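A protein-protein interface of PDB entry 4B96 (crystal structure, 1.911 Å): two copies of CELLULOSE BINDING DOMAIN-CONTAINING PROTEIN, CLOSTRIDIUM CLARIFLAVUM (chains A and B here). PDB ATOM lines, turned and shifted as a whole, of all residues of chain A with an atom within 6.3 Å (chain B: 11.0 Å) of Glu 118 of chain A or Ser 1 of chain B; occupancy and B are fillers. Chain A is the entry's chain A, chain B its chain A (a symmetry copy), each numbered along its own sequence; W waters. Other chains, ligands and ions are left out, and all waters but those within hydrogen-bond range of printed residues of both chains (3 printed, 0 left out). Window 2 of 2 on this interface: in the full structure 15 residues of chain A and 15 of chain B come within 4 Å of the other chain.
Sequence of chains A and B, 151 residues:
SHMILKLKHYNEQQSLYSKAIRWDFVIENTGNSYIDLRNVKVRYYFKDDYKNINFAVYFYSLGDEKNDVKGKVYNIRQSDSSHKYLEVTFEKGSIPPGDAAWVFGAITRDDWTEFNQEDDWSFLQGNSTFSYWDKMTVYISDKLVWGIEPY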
ATOM      1  N   LEU A  16     -11.600  14.081  13.608  1.00  0.00           N
ATOM      2  CA  LEU A  16     -10.450  14.837  14.108  1.00  0.00           C
ATOM      3  C   LEU A  16      -9.323  13.852  14.508  1.00  0.00           C
ATOM      4  O   LEU A  16      -8.161  14.093  14.249  1.00  0.00           O
ATOM      5  CB  LEU A  16     -10.875  15.684  15.323  1.00  0.00           C
ATOM      6  CG  LEU A  16     -11.850  16.827  15.020  1.00  0.00           C
ATOM      7  CD1 LEU A  16     -11.855  17.778  16.182  1.00  0.00           C
ATOM      8  CD2 LEU A  16     -11.388  17.539  13.699  1.00  0.00           C
ATOM      9  N   TYR A  17      -9.677  12.746  15.164  1.00  0.00           N
ATOM     10  CA  TYR A  17      -8.671  11.734  15.507  1.00  0.00           C
ATOM     11  C   TYR A  17      -8.672  10.570  14.519  1.00  0.00           C
ATOM     12  O   TYR A  17      -9.698   9.930  14.319  1.00  0.00           O
ATOM     13  CB  TYR A  17      -8.912  11.230  16.930  1.00  0.00           C
ATOM     14  CG  TYR A  17      -8.686  12.335  17.946  1.00  0.00           C
ATOM     15  CD1 TYR A  17      -7.412  12.636  18.385  1.00  0.00           C
ATOM     16  CD2 TYR A  17      -9.739  13.099  18.437  1.00  0.00           C
ATOM     17  CE1 TYR A  17      -7.173  13.660  19.323  1.00  0.00           C
ATOM     18  CE2 TYR A  17      -9.520  14.131  19.377  1.00  0.00           C
ATOM     19  CZ  TYR A  17      -8.228  14.404  19.805  1.00  0.00           C
ATOM     20  OH  TYR A  17      -7.973  15.413  20.714  1.00  0.00           O
ATOM     21  N   ASN A 116      -4.066  13.841  15.550  1.00  0.00           N
ATOM     22  CA  ASN A 116      -5.121  14.808  15.783  1.00  0.00           C
ATOM     23  C   ASN A 116      -5.042  15.783  14.623  1.00  0.00           C
ATOM     24  O   ASN A 116      -4.079  16.571  14.521  1.00  0.00           O
ATOM     25  CB  ASN A 116      -4.861  15.545  17.116  1.00  0.00           C
ATOM     26  CG  ASN A 116      -5.817  16.746  17.322  1.00  0.00           C
ATOM     27  OD1 ASN A 116      -6.824  16.892  16.616  1.00  0.00           O
ATOM     28  ND2 ASN A 116      -5.488  17.615  18.279  1.00  0.00           N
ATOM     29  N   GLN A 117      -6.008  15.731  13.718  1.00  0.00           N
ATOM     30  CA  GLN A 117      -5.939  16.483  12.509  1.00  0.00           C
ATOM     31  C   GLN A 117      -6.402  17.920  12.683  1.00  0.00           C
ATOM     32  O   GLN A 117      -6.276  18.734  11.751  1.00  0.00           O
ATOM     33  CB  GLN A 117      -6.850  15.841  11.478  1.00  0.00           C
ATOM     34  CG  GLN A 117      -6.499  14.387  11.193  1.00  0.00           C
ATOM     35  CD  GLN A 117      -7.159  13.895   9.883  1.00  0.00           C
ATOM     36  OE1 GLN A 117      -6.637  14.150   8.824  1.00  0.00           O
ATOM     37  NE2 GLN A 117      -8.295  13.220   9.986  1.00  0.00           N
ATOM     38  N   GLU A 118      -6.947  18.211  13.845  1.00  0.00           N
ATOM     39  CA  GLU A 118      -7.620  19.507  14.041  1.00  0.00           C
ATOM     40  C   GLU A 118      -6.722  20.723  13.818  1.00  0.00           C
ATOM     41  O   GLU A 118      -7.198  21.775  13.420  1.00  0.00           O
ATOM     42  CB  GLU A 118      -8.260  19.601  15.418  1.00  0.00           C
ATOM     43  CG  GLU A 118      -9.231  20.809  15.501  1.00  0.00           C
ATOM     44  CD  GLU A 118      -9.968  20.902  16.838  1.00  0.00           C
ATOM     45  OE1 GLU A 118      -9.397  20.468  17.888  1.00  0.00           O
ATOM     46  OE2 GLU A 118     -11.124  21.416  16.819  1.00  0.00           O
ATOM     47  N   ASP A 119      -5.418  20.569  14.081  1.00  0.00           N
ATOM     48  CA  ASP A 119      -4.497  21.683  13.978  1.00  0.00           C
ATOM     49  C   ASP A 119      -3.611  21.548  12.742  1.00  0.00           C
ATOM     50  O   ASP A 119      -2.545  22.194  12.651  1.00  0.00           O
ATOM     51  CB  ASP A 119      -3.663  21.721  15.272  1.00  0.00           C
ATOM     52  CG  ASP A 119      -2.981  20.347  15.597  1.00  0.00           C
ATOM     53  OD1 ASP A 119      -2.971  19.390  14.740  1.00  0.00           O
ATOM     54  OD2 ASP A 119      -2.433  20.236  16.733  1.00  0.00           O
ATOM     55  N   ASP A 120      -4.029  20.723  11.770  1.00  0.00           N
ATOM     56  CA  ASP A 120      -3.212  20.519  10.576  1.00  0.00           C
ATOM     57  C   ASP A 120      -3.632  21.510   9.492  1.00  0.00           C
ATOM     58  O   ASP A 120      -4.828  21.572   9.081  1.00  0.00           O
ATOM     59  CB  ASP A 120      -3.403  19.089  10.023  1.00  0.00           C
ATOM     60  CG  ASP A 120      -2.887  18.017  10.957  1.00  0.00           C
ATOM     61  OD1 ASP A 120      -2.169  18.318  11.941  1.00  0.00           O
ATOM     62  OD2 ASP A 120      -3.184  16.826  10.686  1.00  0.00           O
ATOM     63  N   TRP A 121      -2.685  22.306   9.017  1.00  0.00           N
ATOM     64  CA  TRP A 121      -3.028  23.348   8.033  1.00  0.00           C
ATOM     65  C   TRP A 121      -3.798  22.758   6.809  1.00  0.00           C
ATOM     66  O   TRP A 121      -4.767  23.358   6.330  1.00  0.00           O
ATOM     67  CB  TRP A 121      -1.726  24.033   7.554  1.00  0.00           C
ATOM     68  CG  TRP A 121      -1.883  25.199   6.528  1.00  0.00           C
ATOM     69  CD1 TRP A 121      -1.714  25.130   5.150  1.00  0.00           C
ATOM     70  CD2 TRP A 121      -2.221  26.552   6.821  1.00  0.00           C
ATOM     71  NE1 TRP A 121      -1.948  26.378   4.588  1.00  0.00           N
ATOM     72  CE2 TRP A 121      -2.233  27.266   5.590  1.00  0.00           C
ATOM     73  CE3 TRP A 121      -2.496  27.240   8.013  1.00  0.00           C
ATOM     74  CZ2 TRP A 121      -2.481  28.643   5.517  1.00  0.00           C
ATOM     75  CZ3 TRP A 121      -2.744  28.595   7.944  1.00  0.00           C
ATOM     76  CH2 TRP A 121      -2.750  29.285   6.699  1.00  0.00           C
ATOM     77  N   SER A 122      -3.372  21.615   6.294  1.00  0.00           N
ATOM     78  CA  SER A 122      -3.988  21.122   5.040  1.00  0.00           C
ATOM     79  C   SER A 122      -5.312  20.372   5.235  1.00  0.00           C
ATOM     80  O   SER A 122      -5.894  19.923   4.258  1.00  0.00           O
ATOM     81  CB  SER A 122      -2.988  20.227   4.263  1.00  0.00           C
ATOM     82  OG  SER A 122      -1.919  21.035   3.780  1.00  0.00           O
ATOM     83  N   PHE A 123      -5.745  20.194   6.489  1.00  0.00           N
ATOM     84  CA  PHE A 123      -6.906  19.351   6.808  1.00  0.00           C
ATOM     85  C   PHE A 123      -8.211  19.941   6.244  1.00  0.00           C
ATOM     86  O   PHE A 123      -8.534  21.107   6.503  1.00  0.00           O
ATOM     87  CB  PHE A 123      -7.025  19.196   8.303  1.00  0.00           C
ATOM     88  CG  PHE A 123      -8.203  18.354   8.767  1.00  0.00           C
ATOM     89  CD1 PHE A 123      -8.439  17.058   8.245  1.00  0.00           C
ATOM     90  CD2 PHE A 123      -9.032  18.827   9.741  1.00  0.00           C
ATOM     91  CE1 PHE A 123      -9.519  16.300   8.733  1.00  0.00           C
ATOM     92  CE2 PHE A 123     -10.082  18.066  10.231  1.00  0.00           C
ATOM     93  CZ  PHE A 123     -10.330  16.826   9.709  1.00  0.00           C
ATOM     94  N   LYS A 135      -4.994  25.005   0.495  1.00  0.00           N
ATOM     95  CA  LYS A 135      -4.140  24.799   1.683  1.00  0.00           C
ATOM     96  C   LYS A 135      -3.196  23.635   1.495  1.00  0.00           C
ATOM     97  O   LYS A 135      -2.462  23.244   2.399  1.00  0.00           O
ATOM     98  CB  LYS A 135      -4.967  24.685   2.997  1.00  0.00           C
ATOM     99  CG  LYS A 135      -5.775  25.999   3.244  1.00  0.00           C
ATOM    100  CD  LYS A 135      -6.508  25.916   4.582  1.00  0.00           C
ATOM    101  CE  LYS A 135      -5.564  26.222   5.750  1.00  0.00           C
ATOM    102  NZ  LYS A 135      -6.218  25.828   7.037  1.00  0.00           N
ATOM    103  N   TYR A 151       0.815  30.278   7.740  1.00  0.00           N
ATOM    104  CA  TYR A 151       1.295  31.519   8.320  1.00  0.00           C
ATOM    105  C   TYR A 151       0.516  31.761   9.597  1.00  0.00           C
ATOM    106  O   TYR A 151       0.846  32.662  10.354  1.00  0.00           O
ATOM    107  CB  TYR A 151       1.055  32.639   7.354  1.00  0.00           C
ATOM    108  CG  TYR A 151      -0.418  32.980   7.044  1.00  0.00           C
ATOM    109  CD1 TYR A 151      -1.118  33.921   7.825  1.00  0.00           C
ATOM    110  CD2 TYR A 151      -1.064  32.401   5.951  1.00  0.00           C
ATOM    111  CE1 TYR A 151      -2.455  34.254   7.529  1.00  0.00           C
ATOM    112  CE2 TYR A 151      -2.400  32.688   5.659  1.00  0.00           C
ATOM    113  CZ  TYR A 151      -3.076  33.635   6.429  1.00  0.00           C
ATOM    114  OH  TYR A 151      -4.386  33.948   6.111  1.00  0.00           O
ATOM    115  OXT TYR A 151      -0.454  31.034   9.886  1.00  0.00           O
ATOM    116  N   SER B   1      -3.907  27.199  12.598  1.00  0.00           N
ATOM    117  CA  SER B   1      -4.011  26.300  11.460  1.00  0.00           C
ATOM    118  C   SER B   1      -4.998  26.785  10.415  1.00  0.00           C
ATOM    119  O   SER B   1      -5.228  26.065   9.475  1.00  0.00           O
ATOM    120  CB  SER B   1      -4.360  24.893  11.915  1.00  0.00           C
ATOM    121  OG  SER B   1      -5.728  24.775  12.277  1.00  0.00           O
ATOM    122  N   HIS B   2      -5.534  28.006  10.550  1.00  0.00           N
ATOM    123  CA  HIS B   2      -6.517  28.568   9.620  1.00  0.00           C
ATOM    124  C   HIS B   2      -6.030  29.764   8.820  1.00  0.00           C
ATOM    125  O   HIS B   2      -5.358  30.661   9.369  1.00  0.00           O
ATOM    126  CB  HIS B   2      -7.793  29.000  10.363  1.00  0.00           C
ATOM    127  CG  HIS B   2      -8.457  27.876  11.086  1.00  0.00           C
ATOM    128  ND1 HIS B   2      -9.008  26.793  10.430  1.00  0.00           N
ATOM    129  CD2 HIS B   2      -8.623  27.636  12.409  1.00  0.00           C
ATOM    130  CE1 HIS B   2      -9.491  25.936  11.314  1.00  0.00           C
ATOM    131  NE2 HIS B   2      -9.273  26.425  12.522  1.00  0.00           N
ATOM    132  N   MET B   3      -6.427  29.810   7.541  1.00  0.00           N
ATOM    133  CA  MET B   3      -6.350  31.033   6.741  1.00  0.00           C
ATOM    134  C   MET B   3      -7.268  32.071   7.369  1.00  0.00           C
ATOM    135  O   MET B   3      -8.355  31.723   7.782  1.00  0.00           O
ATOM    136  CB  MET B   3      -6.872  30.771   5.326  1.00  0.00           C
ATOM    137  CG  MET B   3      -6.027  29.948   4.477  1.00  0.00           C
ATOM    138  SD  MET B   3      -7.013  29.475   3.043  1.00  0.00           S
ATOM    139  CE  MET B   3      -7.603  31.106   2.504  1.00  0.00           C
ATOM    140  N   ILE B   4      -6.914  33.351   7.378  1.00  0.00           N
ATOM    141  CA  ILE B   4      -7.825  34.338   7.956  1.00  0.00           C
ATOM    142  C   ILE B   4      -8.244  35.418   6.941  1.00  0.00           C
ATOM    143  O   ILE B   4      -8.991  36.338   7.284  1.00  0.00           O
ATOM    144  CB  ILE B   4      -7.289  34.978   9.291  1.00  0.00           C
ATOM    145  CG1 ILE B   4      -5.879  35.544   9.148  1.00  0.00           C
ATOM    146  CG2 ILE B   4      -7.147  33.902  10.348  1.00  0.00           C
ATOM    147  CD1 ILE B   4      -5.715  36.676   8.287  1.00  0.00           C
ATOM    148  N   LEU B   5      -7.828  35.262   5.696  1.00  0.00           N
ATOM    149  CA  LEU B   5      -8.317  36.208   4.698  1.00  0.00           C
ATOM    150  C   LEU B   5      -8.433  35.592   3.319  1.00  0.00           C
ATOM    151  O   LEU B   5      -7.726  34.613   2.995  1.00  0.00           O
ATOM    152  CB  LEU B   5      -7.464  37.496   4.648  1.00  0.00           C
ATOM    153  CG  LEU B   5      -6.143  37.694   3.956  1.00  0.00           C
ATOM    154  CD1 LEU B   5      -6.207  37.658   2.375  1.00  0.00           C
ATOM    155  CD2 LEU B   5      -5.657  39.088   4.387  1.00  0.00           C
ATOM    156  N   THR B  30     -11.841  36.281   7.313  1.00  0.00           N
ATOM    157  CA  THR B  30     -12.518  35.033   7.685  1.00  0.00           C
ATOM    158  C   THR B  30     -12.087  34.514   9.039  1.00  0.00           C
ATOM    159  O   THR B  30     -12.471  33.409   9.435  1.00  0.00           O
ATOM    160  CB  THR B  30     -12.226  33.915   6.666  1.00  0.00           C
ATOM    161  OG1 THR B  30     -10.795  33.732   6.561  1.00  0.00           O
ATOM    162  CG2 THR B  30     -12.776  34.284   5.291  1.00  0.00           C
ATOM    163  N   GLY B  31     -11.303  35.285   9.798  1.00  0.00           N
ATOM    164  CA  GLY B  31     -10.935  34.810  11.147  1.00  0.00           C
ATOM    165  C   GLY B  31     -11.652  35.530  12.301  1.00  0.00           C
ATOM    166  O   GLY B  31     -12.700  36.127  12.097  1.00  0.00           O
ATOM    167  N   ASN B  32     -11.119  35.437  13.521  1.00  0.00           N
ATOM    168  CA  ASN B  32     -11.789  35.987  14.694  1.00  0.00           C
ATOM    169  C   ASN B  32     -11.148  37.226  15.290  1.00  0.00           C
ATOM    170  O   ASN B  32     -11.571  37.674  16.361  1.00  0.00           O
ATOM    171  CB  ASN B  32     -11.926  34.938  15.776  1.00  0.00           C
ATOM    172  CG  ASN B  32     -12.561  33.676  15.249  1.00  0.00           C
ATOM    173  OD1 ASN B  32     -13.586  33.723  14.545  1.00  0.00           O
ATOM    174  ND2 ASN B  32     -11.924  32.541  15.516  1.00  0.00           N
HETATM  175  O   HOH W   1      -5.212  33.633   3.608  1.00  0.00           O
HETATM  176  O   HOH W   2      -3.106  31.590  10.826  1.00  0.00           O
HETATM  177  O   HOH W   3      -6.731  23.211  10.259  1.00  0.00           O
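The side-chain hydroxyl (OH) of Tyr 151 of chain A lies within hydrogen-bond range of the backbone NH (N) of Ile 4 of chain B (2.9 Å).
The backbone carbonyl oxygen (O) of Ser 1 of chain B is in hydrogen-bond range of the side-chain amino group (NZ) of Lys 135 of chain A (2.6 Å).
O of Ile 4 of chain B is in hydrogen-bond range of N of Thr 30 of chain B (2.9 Å).
The backbone NH (N) of Glu 118 of chain A lies within hydrogen-bond range of the side-chain amide oxygen (OD1) of Asn 116 of chain A (3.1 Å).
NZ of Lys 135 of chain A sits at hydrogen-bond distance from O of Trp 121 of chain A, at 3.0 Å.
The side-chain hydroxyl (OG) of Ser 122 of chain A sits at hydrogen-bond distance from the backbone carbonyl oxygen (O) of Lys 135 of chain A (2.7 Å).
The backbone carbonyl oxygen (O) of Met 3 of chain B sits at hydrogen-bond distance from the side-chain hydroxyl (OG1) of Thr 30 of chain B.
OG1 of Thr 30 of chain B lies within hydrogen-bond range of N of Leu 5 of chain B.
Among the printed residues, pairs that only touch across the chains: Glu 118 of chain A with Ser 1 of chain B, Asp 119 of chain A with Ser 1 of chain B, Trp 121 of chain A with Ser 1 of chain B, Trp 121 of chain A with His 2 of chain B, Trp 121 of chain A with Met 3 of chain B, Lys 135 of chain A with His 2 of chain B, Lys 135 of chain A with Met 3 of chain B, Tyr 151 of chain A with Met 3 of chain B and Tyr 151 of chain A with Leu 5 of chain B.
Leu 16 of chain A touches none of the printed residues of chain B.
Tyr 17 of chain A touches none of the printed residues of chain B.
No residue of chain B comes within 4 Å of Asn 116 of chain A.
No residue of chain B comes within 4 Å of Gln 117 of chain A.
Glu 118 of chain A touches just one residue of chain B: Ser 1 (3.5 Å).
Asp 119 of chain A touches one residue of chain B.
Of chain B, only Ser 1, His 2 and Met 3 come within 4 Å of Trp 121 of chain A.
Printed residues of chain A within 4 Å of Ser 1 of chain B: Glu 118 (3.5 Å), Asp 119 (3.3 Å), Trp 121 (3.3 Å) and Lys 135 (2.6 Å).
Of the printed residues of chain A, Met 3 of chain B touches Trp 121 (3.8 Å), Lys 135 (3.7 Å) and Tyr 151 (3.6 Å).
Printed residues of chain A within 4 Å of Leu 5 of chain B: Tyr 151.
Asn 32 of chain B touches none of the printed residues of chain A.
The nearest residue of chain A that does not touch Ser 1 of chain B is Asp 120 of chain A (4.2 Å).
Of the 12 printed residues of chain A, 5 touch a printed residue of chain B.
Hydrophobic or aromatic side chains of chain A that line the printed part of chain B: Trp 121 and Tyr 151.
Of the 8 printed residues of chain B, 5 touch a printed residue of chain A.
Hydrophobic or aromatic side chains of chain B that line the printed part of chain A: Met 3 and Ile 4.
Among the printed residues, 11 pairs touch across the chains.
No position is printed for both chains.
Of the 11 pairs that touch across the chains among the printed residues, none has its exchanged pair printed and touching as well.
Water W1 bridges OH of Tyr 151 of chain A (2.7 Å) and O of Leu 5 of chain B (2.8 Å).
Water W3 bridges the side-chain hydroxyl of Ser 1 of chain B (2.7 Å) and the backbone carbonyl oxygen of Asp 120 of chain A (2.8 Å).
Water W2 bridges the backbone carbonyl oxygen (O) of His 2 of chain B (2.8 Å) and the chain-end carboxylate (OXT) of Tyr 151 of chain A (2.9 Å).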
